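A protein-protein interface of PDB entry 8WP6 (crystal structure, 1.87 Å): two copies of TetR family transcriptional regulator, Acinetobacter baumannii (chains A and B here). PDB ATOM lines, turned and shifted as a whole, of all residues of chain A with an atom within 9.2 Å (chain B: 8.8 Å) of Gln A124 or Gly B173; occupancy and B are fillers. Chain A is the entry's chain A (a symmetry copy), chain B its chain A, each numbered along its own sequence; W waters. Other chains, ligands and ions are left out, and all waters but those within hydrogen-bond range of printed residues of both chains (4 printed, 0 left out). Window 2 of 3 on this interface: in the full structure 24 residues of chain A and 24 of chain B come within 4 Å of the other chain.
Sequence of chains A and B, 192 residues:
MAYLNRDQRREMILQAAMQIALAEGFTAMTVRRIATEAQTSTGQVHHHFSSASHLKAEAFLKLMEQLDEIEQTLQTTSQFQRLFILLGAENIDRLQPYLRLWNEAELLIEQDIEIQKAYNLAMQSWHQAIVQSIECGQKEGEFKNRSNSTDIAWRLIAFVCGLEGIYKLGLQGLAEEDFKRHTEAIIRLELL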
ATOM      1  N   LEU A  61      -6.396   7.327  17.938  1.00  0.00           N
ATOM      2  CA  LEU A  61      -5.197   7.129  18.745  1.00  0.00           C
ATOM      3  C   LEU A  61      -5.433   6.110  19.851  1.00  0.00           C
ATOM      4  O   LEU A  61      -4.534   5.327  20.179  1.00  0.00           O
ATOM      5  CB  LEU A  61      -4.734   8.462  19.333  1.00  0.00           C
ATOM      6  CG  LEU A  61      -4.003   9.396  18.371  1.00  0.00           C
ATOM      7  CD1 LEU A  61      -3.692  10.722  19.052  1.00  0.00           C
ATOM      8  CD2 LEU A  61      -2.733   8.743  17.845  1.00  0.00           C
ATOM      9  N   TRP A 102      -6.268   2.069  10.082  1.00  0.00           N
ATOM     10  CA  TRP A 102      -4.971   2.699   9.862  1.00  0.00           C
ATOM     11  C   TRP A 102      -4.810   3.127   8.408  1.00  0.00           C
ATOM     12  O   TRP A 102      -4.415   4.264   8.125  1.00  0.00           O
ATOM     13  CB  TRP A 102      -3.856   1.738  10.279  1.00  0.00           C
ATOM     14  CG  TRP A 102      -2.476   2.146   9.845  1.00  0.00           C
ATOM     15  CD1 TRP A 102      -1.844   1.793   8.688  1.00  0.00           C
ATOM     16  CD2 TRP A 102      -1.552   2.967  10.572  1.00  0.00           C
ATOM     17  NE1 TRP A 102      -0.586   2.349   8.645  1.00  0.00           N
ATOM     18  CE2 TRP A 102      -0.381   3.074   9.788  1.00  0.00           C
ATOM     19  CE3 TRP A 102      -1.599   3.624  11.806  1.00  0.00           C
ATOM     20  CZ2 TRP A 102       0.729   3.809  10.198  1.00  0.00           C
ATOM     21  CZ3 TRP A 102      -0.496   4.357  12.211  1.00  0.00           C
ATOM     22  CH2 TRP A 102       0.654   4.442  11.409  1.00  0.00           C
ATOM     23  N   LYS A 117      -2.272  15.072  12.359  1.00  0.00           N
ATOM     24  CA  LYS A 117      -1.413  15.086  13.538  1.00  0.00           C
ATOM     25  C   LYS A 117      -1.429  13.745  14.262  1.00  0.00           C
ATOM     26  O   LYS A 117      -0.386  13.277  14.738  1.00  0.00           O
ATOM     27  CB  LYS A 117      -1.841  16.210  14.481  1.00  0.00           C
ATOM     28  CG  LYS A 117      -1.499  17.608  13.962  1.00  0.00           C
ATOM     29  CD  LYS A 117      -1.892  18.686  14.966  1.00  0.00           C
ATOM     30  CE  LYS A 117      -3.347  18.553  15.385  1.00  0.00           C
ATOM     31  NZ  LYS A 117      -3.835  19.759  16.117  1.00  0.00           N
ATOM     32  N   ALA A 118      -2.601  13.114  14.367  1.00  0.00           N
ATOM     33  CA  ALA A 118      -2.692  11.857  15.107  1.00  0.00           C
ATOM     34  C   ALA A 118      -1.967  10.736  14.377  1.00  0.00           C
ATOM     35  O   ALA A 118      -1.358   9.869  15.012  1.00  0.00           O
ATOM     36  CB  ALA A 118      -4.158  11.484  15.334  1.00  0.00           C
ATOM     37  N   TYR A 119      -2.036  10.732  13.043  1.00  0.00           N
ATOM     38  CA  TYR A 119      -1.339   9.709  12.267  1.00  0.00           C
ATOM     39  C   TYR A 119       0.165   9.786  12.491  1.00  0.00           C
ATOM     40  O   TYR A 119       0.835   8.755  12.625  1.00  0.00           O
ATOM     41  CB  TYR A 119      -1.670   9.867  10.783  1.00  0.00           C
ATOM     42  CG  TYR A 119      -1.132   8.749   9.910  1.00  0.00           C
ATOM     43  CD1 TYR A 119      -1.864   7.583   9.709  1.00  0.00           C
ATOM     44  CD2 TYR A 119       0.110   8.853   9.304  1.00  0.00           C
ATOM     45  CE1 TYR A 119      -1.379   6.560   8.915  1.00  0.00           C
ATOM     46  CE2 TYR A 119       0.605   7.832   8.507  1.00  0.00           C
ATOM     47  CZ  TYR A 119      -0.146   6.688   8.319  1.00  0.00           C
ATOM     48  OH  TYR A 119       0.337   5.670   7.530  1.00  0.00           O
ATOM     49  N   ASN A 120       0.712  11.002  12.544  1.00  0.00           N
ATOM     50  CA  ASN A 120       2.145  11.157  12.786  1.00  0.00           C
ATOM     51  C   ASN A 120       2.525  10.716  14.191  1.00  0.00           C
ATOM     52  O   ASN A 120       3.592  10.124  14.394  1.00  0.00           O
ATOM     53  CB  ASN A 120       2.561  12.608  12.548  1.00  0.00           C
ATOM     54  CG  ASN A 120       2.791  12.912  11.085  1.00  0.00           C
ATOM     55  OD1 ASN A 120       2.617  12.049  10.225  1.00  0.00           O
ATOM     56  ND2 ASN A 120       3.167  14.149  10.791  1.00  0.00           N
ATOM     57  N   LEU A 121       1.679  11.013  15.180  1.00  0.00           N
ATOM     58  CA  LEU A 121       1.937  10.525  16.533  1.00  0.00           C
ATOM     59  C   LEU A 121       1.962   9.002  16.573  1.00  0.00           C
ATOM     60  O   LEU A 121       2.812   8.405  17.242  1.00  0.00           O
ATOM     61  CB  LEU A 121       0.879  11.058  17.499  1.00  0.00           C
ATOM     62  CG  LEU A 121       1.077  12.478  18.028  1.00  0.00           C
ATOM     63  CD1 LEU A 121      -0.252  13.032  18.529  1.00  0.00           C
ATOM     64  CD2 LEU A 121       2.142  12.513  19.117  1.00  0.00           C
ATOM     65  N   ALA A 122       1.033   8.355  15.864  1.00  0.00           N
ATOM     66  CA  ALA A 122       1.021   6.896  15.812  1.00  0.00           C
ATOM     67  C   ALA A 122       2.251   6.358  15.092  1.00  0.00           C
ATOM     68  O   ALA A 122       2.779   5.301  15.457  1.00  0.00           O
ATOM     69  CB  ALA A 122      -0.260   6.407  15.129  1.00  0.00           C
ATOM     70  N   MET A 123       2.721   7.072  14.064  1.00  0.00           N
ATOM     71  CA  MET A 123       3.939   6.665  13.365  1.00  0.00           C
ATOM     72  C   MET A 123       5.147   6.705  14.294  1.00  0.00           C
ATOM     73  O   MET A 123       5.970   5.781  14.301  1.00  0.00           O
ATOM     74  CB  MET A 123       4.174   7.558  12.144  1.00  0.00           C
ATOM     75  CG  MET A 123       3.282   7.267  10.938  1.00  0.00           C
ATOM     76  SD  MET A 123       3.702   5.725  10.077  1.00  0.00           S
ATOM     77  CE  MET A 123       5.482   5.733  10.227  1.00  0.00           C
ATOM     78  N   GLN A 124       5.282   7.779  15.073  1.00  0.00           N
ATOM     79  CA  GLN A 124       6.389   7.860  16.022  1.00  0.00           C
ATOM     80  C   GLN A 124       6.282   6.778  17.088  1.00  0.00           C
ATOM     81  O   GLN A 124       7.298   6.209  17.507  1.00  0.00           O
ATOM     82  CB  GLN A 124       6.436   9.242  16.675  1.00  0.00           C
ATOM     83  CG  GLN A 124       6.587  10.397  15.697  1.00  0.00           C
ATOM     84  CD  GLN A 124       8.035  10.702  15.359  1.00  0.00           C
ATOM     85  OE1 GLN A 124       8.952  10.029  15.832  1.00  0.00           O
ATOM     86  NE2 GLN A 124       8.248  11.728  14.536  1.00  0.00           N
ATOM     87  N   SER A 125       5.061   6.489  17.545  1.00  0.00           N
ATOM     88  CA  SER A 125       4.865   5.421  18.519  1.00  0.00           C
ATOM     89  C   SER A 125       5.275   4.073  17.940  1.00  0.00           C
ATOM     90  O   SER A 125       5.882   3.246  18.633  1.00  0.00           O
ATOM     91  CB  SER A 125       3.406   5.383  18.970  1.00  0.00           C
ATOM     92  OG  SER A 125       3.100   6.500  19.788  1.00  0.00           O
ATOM     93  N   TRP A 126       4.944   3.841  16.668  1.00  0.00           N
ATOM     94  CA  TRP A 126       5.337   2.615  15.982  1.00  0.00           C
ATOM     95  C   TRP A 126       6.853   2.514  15.881  1.00  0.00           C
ATOM     96  O   TRP A 126       7.439   1.463  16.161  1.00  0.00           O
ATOM     97  CB  TRP A 126       4.703   2.598  14.594  1.00  0.00           C
ATOM     98  CG  TRP A 126       4.832   1.322  13.811  1.00  0.00           C
ATOM     99  CD1 TRP A 126       5.088   0.068  14.292  1.00  0.00           C
ATOM    100  CD2 TRP A 126       4.730   1.195  12.388  1.00  0.00           C
ATOM    101  NE1 TRP A 126       5.138  -0.836  13.250  1.00  0.00           N
ATOM    102  CE2 TRP A 126       4.919  -0.165  12.073  1.00  0.00           C
ATOM    103  CE3 TRP A 126       4.490   2.103  11.350  1.00  0.00           C
ATOM    104  CZ2 TRP A 126       4.876  -0.641  10.764  1.00  0.00           C
ATOM    105  CZ3 TRP A 126       4.451   1.630  10.048  1.00  0.00           C
ATOM    106  CH2 TRP A 126       4.640   0.267   9.768  1.00  0.00           C
ATOM    107  N   HIS A 127       7.505   3.612  15.479  1.00  0.00           N
ATOM    108  CA  HIS A 127       8.961   3.629  15.394  1.00  0.00           C
ATOM    109  C   HIS A 127       9.595   3.345  16.750  1.00  0.00           C
ATOM    110  O   HIS A 127      10.582   2.604  16.841  1.00  0.00           O
ATOM    111  CB  HIS A 127       9.434   4.981  14.850  1.00  0.00           C
ATOM    112  CG  HIS A 127      10.901   5.234  15.031  1.00  0.00           C
ATOM    113  ND1 HIS A 127      11.846   4.797  14.127  1.00  0.00           N
ATOM    114  CD2 HIS A 127      11.583   5.880  16.005  1.00  0.00           C
ATOM    115  CE1 HIS A 127      13.048   5.160  14.540  1.00  0.00           C
ATOM    116  NE2 HIS A 127      12.916   5.818  15.678  1.00  0.00           N
ATOM    117  N   GLN A 128       9.038   3.914  17.819  1.00  0.00           N
ATOM    118  CA  GLN A 128       9.630   3.698  19.134  1.00  0.00           C
ATOM    119  C   GLN A 128       9.434   2.262  19.610  1.00  0.00           C
ATOM    120  O   GLN A 128      10.288   1.727  20.322  1.00  0.00           O
ATOM    121  CB  GLN A 128       9.049   4.692  20.143  1.00  0.00           C
ATOM    122  CG  GLN A 128       9.669   4.594  21.535  1.00  0.00           C
ATOM    123  CD  GLN A 128      11.190   4.483  21.495  1.00  0.00           C
ATOM    124  OE1 GLN A 128      11.878   5.367  20.978  1.00  0.00           O
ATOM    125  NE2 GLN A 128      11.721   3.397  22.052  1.00  0.00           N
ATOM    126  N   ALA A 129       8.328   1.619  19.226  1.00  0.00           N
ATOM    127  CA  ALA A 129       8.143   0.215  19.579  1.00  0.00           C
ATOM    128  C   ALA A 129       9.118  -0.688  18.833  1.00  0.00           C
ATOM    129  O   ALA A 129       9.524  -1.732  19.358  1.00  0.00           O
ATOM    130  CB  ALA A 129       6.703  -0.216  19.304  1.00  0.00           C
ATOM    131  N   ILE A 130       9.500  -0.314  17.610  1.00  0.00           N
ATOM    132  CA  ILE A 130      10.493  -1.090  16.877  1.00  0.00           C
ATOM    133  C   ILE A 130      11.879  -0.864  17.463  1.00  0.00           C
ATOM    134  O   ILE A 130      12.660  -1.810  17.632  1.00  0.00           O
ATOM    135  CB  ILE A 130      10.434  -0.738  15.379  1.00  0.00           C
ATOM    136  CG1 ILE A 130       9.022  -0.983  14.847  1.00  0.00           C
ATOM    137  CG2 ILE A 130      11.487  -1.519  14.588  1.00  0.00           C
ATOM    138  CD1 ILE A 130       8.829  -2.326  14.202  1.00  0.00           C
ATOM    139  N   VAL A 131      12.197   0.389  17.801  1.00  0.00           N
ATOM    140  CA  VAL A 131      13.458   0.702  18.474  1.00  0.00           C
ATOM    141  C   VAL A 131      13.595  -0.121  19.747  1.00  0.00           C
ATOM    142  O   VAL A 131      14.648  -0.705  20.024  1.00  0.00           O
ATOM    143  CB  VAL A 131      13.541   2.209  18.779  1.00  0.00           C
ATOM    144  CG1 VAL A 131      14.728   2.506  19.687  1.00  0.00           C
ATOM    145  CG2 VAL A 131      13.620   3.024  17.485  1.00  0.00           C
ATOM    146  N   GLN A 132      12.528  -0.167  20.547  1.00  0.00           N
ATOM    147  CA  GLN A 132      12.571  -0.899  21.809  1.00  0.00           C
ATOM    148  C   GLN A 132      12.821  -2.385  21.580  1.00  0.00           C
ATOM    149  O   GLN A 132      13.595  -3.013  22.312  1.00  0.00           O
ATOM    150  CB  GLN A 132      11.268  -0.680  22.574  1.00  0.00           C
ATOM    151  CG  GLN A 132      11.244  -1.272  23.963  1.00  0.00           C
ATOM    152  CD  GLN A 132      10.140  -2.295  24.123  1.00  0.00           C
ATOM    153  OE1 GLN A 132      10.166  -3.355  23.496  1.00  0.00           O
ATOM    154  NE2 GLN A 132       9.149  -1.972  24.950  1.00  0.00           N
ATOM    155  N   THR A 150      17.865   3.448  15.991  1.00  0.00           N
ATOM    156  CA  THR A 150      16.929   4.412  15.420  1.00  0.00           C
ATOM    157  C   THR A 150      16.958   4.361  13.896  1.00  0.00           C
ATOM    158  O   THR A 150      15.906   4.425  13.246  1.00  0.00           O
ATOM    159  CB  THR A 150      17.249   5.819  15.926  1.00  0.00           C
ATOM    160  OG1 THR A 150      17.078   5.863  17.348  1.00  0.00           O
ATOM    161  CG2 THR A 150      16.326   6.848  15.285  1.00  0.00           C
ATOM    162  N   ASP A 151      18.152   4.220  13.315  1.00  0.00           N
ATOM    163  CA  ASP A 151      18.287   4.135  11.863  1.00  0.00           C
ATOM    164  C   ASP A 151      17.635   2.872  11.319  1.00  0.00           C
ATOM    165  O   ASP A 151      16.933   2.914  10.301  1.00  0.00           O
ATOM    166  CB  ASP A 151      19.763   4.166  11.473  1.00  0.00           C
ATOM    167  CG  ASP A 151      20.338   5.565  11.460  1.00  0.00           C
ATOM    168  OD1 ASP A 151      19.556   6.533  11.440  1.00  0.00           O
ATOM    169  OD2 ASP A 151      21.581   5.692  11.476  1.00  0.00           O
ATOM    170  N   ALA A 153      15.235   1.069  12.653  1.00  0.00           N
ATOM    171  CA  ALA A 153      13.783   1.115  12.802  1.00  0.00           C
ATOM    172  C   ALA A 153      13.125   1.911  11.682  1.00  0.00           C
ATOM    173  O   ALA A 153      12.095   1.493  11.140  1.00  0.00           O
ATOM    174  CB  ALA A 153      13.407   1.704  14.161  1.00  0.00           C
ATOM    175  N   TRP A 154      13.683   3.076  11.335  1.00  0.00           N
ATOM    176  CA  TRP A 154      13.097   3.844  10.238  1.00  0.00           C
ATOM    177  C   TRP A 154      13.217   3.091   8.919  1.00  0.00           C
ATOM    178  O   TRP A 154      12.298   3.128   8.091  1.00  0.00           O
ATOM    179  CB  TRP A 154      13.747   5.228  10.120  1.00  0.00           C
ATOM    180  CG  TRP A 154      13.246   6.247  11.127  1.00  0.00           C
ATOM    181  CD1 TRP A 154      14.007   6.994  11.980  1.00  0.00           C
ATOM    182  CD2 TRP A 154      11.880   6.610  11.388  1.00  0.00           C
ATOM    183  NE1 TRP A 154      13.204   7.807  12.746  1.00  0.00           N
ATOM    184  CE2 TRP A 154      11.896   7.590  12.404  1.00  0.00           C
ATOM    185  CE3 TRP A 154      10.648   6.207  10.862  1.00  0.00           C
ATOM    186  CZ2 TRP A 154      10.731   8.168  12.903  1.00  0.00           C
ATOM    187  CZ3 TRP A 154       9.490   6.785  11.360  1.00  0.00           C
ATOM    188  CH2 TRP A 154       9.542   7.753  12.372  1.00  0.00           C
ATOM    189  N   ILE A 157      10.502   0.363   8.883  1.00  0.00           N
ATOM    190  CA  ILE A 157       9.194   0.957   8.620  1.00  0.00           C
ATOM    191  C   ILE A 157       9.101   1.397   7.166  1.00  0.00           C
ATOM    192  O   ILE A 157       8.096   1.150   6.487  1.00  0.00           O
ATOM    193  CB  ILE A 157       8.935   2.122   9.591  1.00  0.00           C
ATOM    194  CG1 ILE A 157       8.596   1.578  10.980  1.00  0.00           C
ATOM    195  CG2 ILE A 157       7.816   3.041   9.060  1.00  0.00           C
ATOM    196  CD1 ILE A 157       8.405   2.653  12.021  1.00  0.00           C
ATOM    197  N   ILE B 166       7.550   8.216   3.569  1.00  0.00           N
ATOM    198  CA  ILE B 166       7.600   8.629   4.967  1.00  0.00           C
ATOM    199  C   ILE B 166       8.077  10.074   5.077  1.00  0.00           C
ATOM    200  O   ILE B 166       7.646  10.822   5.966  1.00  0.00           O
ATOM    201  CB  ILE B 166       8.494   7.666   5.773  1.00  0.00           C
ATOM    202  CG1 ILE B 166       7.866   6.274   5.853  1.00  0.00           C
ATOM    203  CG2 ILE B 166       8.632   8.148   7.188  1.00  0.00           C
ATOM    204  CD1 ILE B 166       6.362   6.279   5.909  1.00  0.00           C
ATOM    205  N   TYR B 167       8.971  10.495   4.173  1.00  0.00           N
ATOM    206  CA  TYR B 167       9.373  11.901   4.121  1.00  0.00           C
ATOM    207  C   TYR B 167       8.183  12.823   3.885  1.00  0.00           C
ATOM    208  O   TYR B 167       8.149  13.948   4.401  1.00  0.00           O
ATOM    209  CB  TYR B 167      10.409  12.117   3.019  1.00  0.00           C
ATOM    210  CG  TYR B 167      11.754  11.515   3.315  1.00  0.00           C
ATOM    211  CD1 TYR B 167      12.158  11.277   4.622  1.00  0.00           C
ATOM    212  CD2 TYR B 167      12.620  11.173   2.287  1.00  0.00           C
ATOM    213  CE1 TYR B 167      13.393  10.721   4.897  1.00  0.00           C
ATOM    214  CE2 TYR B 167      13.857  10.612   2.554  1.00  0.00           C
ATOM    215  CZ  TYR B 167      14.236  10.392   3.856  1.00  0.00           C
ATOM    216  OH  TYR B 167      15.469   9.835   4.118  1.00  0.00           O
ATOM    217  N   LEU B 169       5.379  12.718   5.084  1.00  0.00           N
ATOM    218  CA  LEU B 169       4.541  12.886   6.264  1.00  0.00           C
ATOM    219  C   LEU B 169       4.921  14.112   7.078  1.00  0.00           C
ATOM    220  O   LEU B 169       4.074  14.651   7.799  1.00  0.00           O
ATOM    221  CB  LEU B 169       4.623  11.635   7.138  1.00  0.00           C
ATOM    222  CG  LEU B 169       4.030  10.366   6.520  1.00  0.00           C
ATOM    223  CD1 LEU B 169       4.160   9.195   7.487  1.00  0.00           C
ATOM    224  CD2 LEU B 169       2.578  10.565   6.128  1.00  0.00           C
ATOM    225  N   GLY B 170       6.165  14.572   6.974  1.00  0.00           N
ATOM    226  CA  GLY B 170       6.627  15.668   7.800  1.00  0.00           C
ATOM    227  C   GLY B 170       6.788  15.260   9.251  1.00  0.00           C
ATOM    228  O   GLY B 170       6.385  15.996  10.157  1.00  0.00           O
ATOM    229  N   LEU B 171       7.372  14.085   9.485  1.00  0.00           N
ATOM    230  CA  LEU B 171       7.686  13.635  10.831  1.00  0.00           C
ATOM    231  C   LEU B 171       8.838  14.456  11.408  1.00  0.00           C
ATOM    232  O   LEU B 171       9.634  15.055  10.681  1.00  0.00           O
ATOM    233  CB  LEU B 171       8.040  12.148  10.824  1.00  0.00           C
ATOM    234  CG  LEU B 171       6.893  11.233  10.396  1.00  0.00           C
ATOM    235  CD1 LEU B 171       7.383   9.822  10.151  1.00  0.00           C
ATOM    236  CD2 LEU B 171       5.810  11.238  11.462  1.00  0.00           C
ATOM    237  N   GLN B 172       8.928  14.469  12.739  1.00  0.00           N
ATOM    238  CA  GLN B 172       9.817  15.400  13.426  1.00  0.00           C
ATOM    239  C   GLN B 172      11.223  14.868  13.673  1.00  0.00           C
ATOM    240  O   GLN B 172      12.141  15.672  13.869  1.00  0.00           O
ATOM    241  CB  GLN B 172       9.207  15.827  14.763  1.00  0.00           C
ATOM    242  CG  GLN B 172       7.908  16.588  14.601  1.00  0.00           C
ATOM    243  CD  GLN B 172       8.115  18.087  14.658  1.00  0.00           C
ATOM    244  OE1 GLN B 172       8.962  18.633  13.951  1.00  0.00           O
ATOM    245  NE2 GLN B 172       7.342  18.763  15.500  1.00  0.00           N
ATOM    246  N   GLY B 173      11.429  13.556  13.680  1.00  0.00           N
ATOM    247  CA  GLY B 173      12.765  13.060  13.959  1.00  0.00           C
ATOM    248  C   GLY B 173      13.455  12.443  12.762  1.00  0.00           C
ATOM    249  O   GLY B 173      14.310  11.565  12.914  1.00  0.00           O
ATOM    250  N   LEU B 174      13.103  12.897  11.564  1.00  0.00           N
ATOM    251  CA  LEU B 174      13.517  12.238  10.332  1.00  0.00           C
ATOM    252  C   LEU B 174      14.050  13.278   9.359  1.00  0.00           C
ATOM    253  O   LEU B 174      13.303  14.157   8.915  1.00  0.00           O
ATOM    254  CB  LEU B 174      12.351  11.470   9.712  1.00  0.00           C
ATOM    255  CG  LEU B 174      12.697  10.542   8.554  1.00  0.00           C
ATOM    256  CD1 LEU B 174      13.737   9.522   8.974  1.00  0.00           C
ATOM    257  CD2 LEU B 174      11.444   9.865   8.069  1.00  0.00           C
ATOM    258  N   ALA B 175      15.331  13.171   9.020  1.00  0.00           N
ATOM    259  CA  ALA B 175      15.993  14.133   8.150  1.00  0.00           C
ATOM    260  C   ALA B 175      16.011  13.599   6.722  1.00  0.00           C
ATOM    261  O   ALA B 175      16.560  12.522   6.465  1.00  0.00           O
ATOM    262  CB  ALA B 175      17.413  14.415   8.640  1.00  0.00           C
ATOM    263  N   GLU B 176      15.412  14.362   5.799  1.00  0.00           N
ATOM    264  CA  GLU B 176      15.414  13.985   4.388  1.00  0.00           C
ATOM    265  C   GLU B 176      16.827  13.822   3.847  1.00  0.00           C
ATOM    266  O   GLU B 176      17.054  13.026   2.929  1.00  0.00           O
ATOM    267  CB  GLU B 176      14.668  15.037   3.565  1.00  0.00           C
ATOM    268  CG  GLU B 176      13.176  15.130   3.841  1.00  0.00           C
ATOM    269  CD  GLU B 176      12.414  15.778   2.696  1.00  0.00           C
ATOM    270  OE1 GLU B 176      13.004  15.964   1.608  1.00  0.00           O
ATOM    271  OE2 GLU B 176      11.230  16.115   2.886  1.00  0.00           O
ATOM    272  N   ASP B 178      19.232  12.297   4.918  1.00  0.00           N
ATOM    273  CA  ASP B 178      19.790  10.977   5.190  1.00  0.00           C
ATOM    274  C   ASP B 178      19.445   9.947   4.118  1.00  0.00           C
ATOM    275  O   ASP B 178      19.849   8.787   4.259  1.00  0.00           O
ATOM    276  CB  ASP B 178      19.296  10.463   6.545  1.00  0.00           C
ATOM    277  CG  ASP B 178      19.963  11.157   7.713  1.00  0.00           C
ATOM    278  OD1 ASP B 178      21.030  11.772   7.509  1.00  0.00           O
ATOM    279  OD2 ASP B 178      19.425  11.077   8.836  1.00  0.00           O
ATOM    280  N   ARG B 181      22.420   8.013   2.595  1.00  0.00           N
ATOM    281  CA  ARG B 181      23.040   7.155   3.598  1.00  0.00           C
ATOM    282  C   ARG B 181      22.217   5.893   3.844  1.00  0.00           C
ATOM    283  O   ARG B 181      22.770   4.790   3.932  1.00  0.00           O
ATOM    284  CB  ARG B 181      23.225   7.944   4.894  1.00  0.00           C
ATOM    285  CG  ARG B 181      23.608   7.120   6.096  1.00  0.00           C
ATOM    286  CD  ARG B 181      24.084   8.019   7.225  1.00  0.00           C
ATOM    287  NE  ARG B 181      22.963   8.534   8.007  1.00  0.00           N
ATOM    288  CZ  ARG B 181      22.339   7.857   8.960  1.00  0.00           C
ATOM    289  NH1 ARG B 181      22.686   6.618   9.268  1.00  0.00           N
ATOM    290  NH2 ARG B 181      21.341   8.438   9.621  1.00  0.00           N
ATOM    291  N   HIS B 182      20.896   6.033   3.961  1.00  0.00           N
ATOM    292  CA  HIS B 182      20.043   4.863   4.150  1.00  0.00           C
ATOM    293  C   HIS B 182      20.044   3.973   2.914  1.00  0.00           C
ATOM    294  O   HIS B 182      20.128   2.743   3.026  1.00  0.00           O
ATOM    295  CB  HIS B 182      18.618   5.300   4.483  1.00  0.00           C
ATOM    296  CG  HIS B 182      18.456   5.831   5.874  1.00  0.00           C
ATOM    297  ND1 HIS B 182      18.959   5.187   6.980  1.00  0.00           N
ATOM    298  CD2 HIS B 182      17.847   6.951   6.331  1.00  0.00           C
ATOM    299  CE1 HIS B 182      18.668   5.887   8.064  1.00  0.00           C
ATOM    300  NE2 HIS B 182      17.998   6.962   7.696  1.00  0.00           N
HETATM  301  O   HOH W   1       6.116  13.808  14.288  1.00  0.00           O
HETATM  302  O   HOH W   2       3.358  17.154   9.363  1.00  0.00           O
HETATM  303  O   HOH W   3       5.442  15.903  12.551  1.00  0.00           O
HETATM  304  O   HOH W   4      14.170   9.700  14.681  1.00  0.00           O
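NH1 of Arg B181 lies within salt-bridge range of OD2 of Asp A151, 2.6 Å away. The side-chain amide nitrogen (ND2) of Asn A120 lies within hydrogen-bond range of the backbone carbonyl oxygen (O) of Leu B169, at 3.2 Å. NE2 of Gln A124 sits close to N of Gln B172 (3.3 Å).
The side-chain carboxylate (OD2) of Asp B178 is in salt-bridge range of the guanidinium group (NH2) of Arg B181 (3.4 Å).
Among the printed residues, merely in contact across the chains: Tyr A119 with Leu B169, Asn A120 with Gly B170, Asn A120 with Leu B171, Gln A124 with Leu B171, Gln A124 with Gly B173, Asp A151 with His B182, Trp A154 with Leu B171, Trp A154 with Gly B173 and Trp A154 with Leu B174.
Gly B173 touches two residues of chain A. No residue of chain B comes within 4 Å of Ser A125. Printed residues of chain B within 4 Å of Tyr A119: Leu B169. Of the printed residues of chain A, Leu B174 touches Trp A154. Of the printed residues of chain A, Gln B172 touches Gln A124 (3.3 Å). Of the printed residues of chain B, Asn A120 touches Leu B169 (3.2 Å), Gly B170 (3.8 Å) and Leu B171 (3.5 Å). The nearest residue of chain A that does not touch Gly B173 is Thr A150 (5.7 Å). The nearest printed residue of chain A that does not touch Arg B181 is Thr A150 (7.4 Å).
Of the 13 printed residues of chain B, 8 touch a printed residue of chain A. Hydrophobic or aromatic side chains of chain B that line the printed part of chain A: Leu B169, Leu B171, Leu B174 and His B182. Hydrophobic or aromatic side chains of chain A within 4 Å of the printed part of chain B: Tyr A119 and Trp A154.
No position is printed for both chains.
Water W4 lies within hydrogen-bond range of O of Gly B173 (2.6 Å) and NE1 of Trp A154 (2.9 Å). Water W3 lies within hydrogen-bond range of O of Gly B170 (2.6 Å) and ND2 of Asn A120 (3.4 Å). Water W1 bridges NE2 of Gln A124 (3.0 Å) and N of Gln B172 (3.3 Å). Water W2 lies within hydrogen-bond range of O of Leu B169 (3.0 Å), ND2 of Asn A120 (3.3 Å) and O of Gly B170 (3.3 Å).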
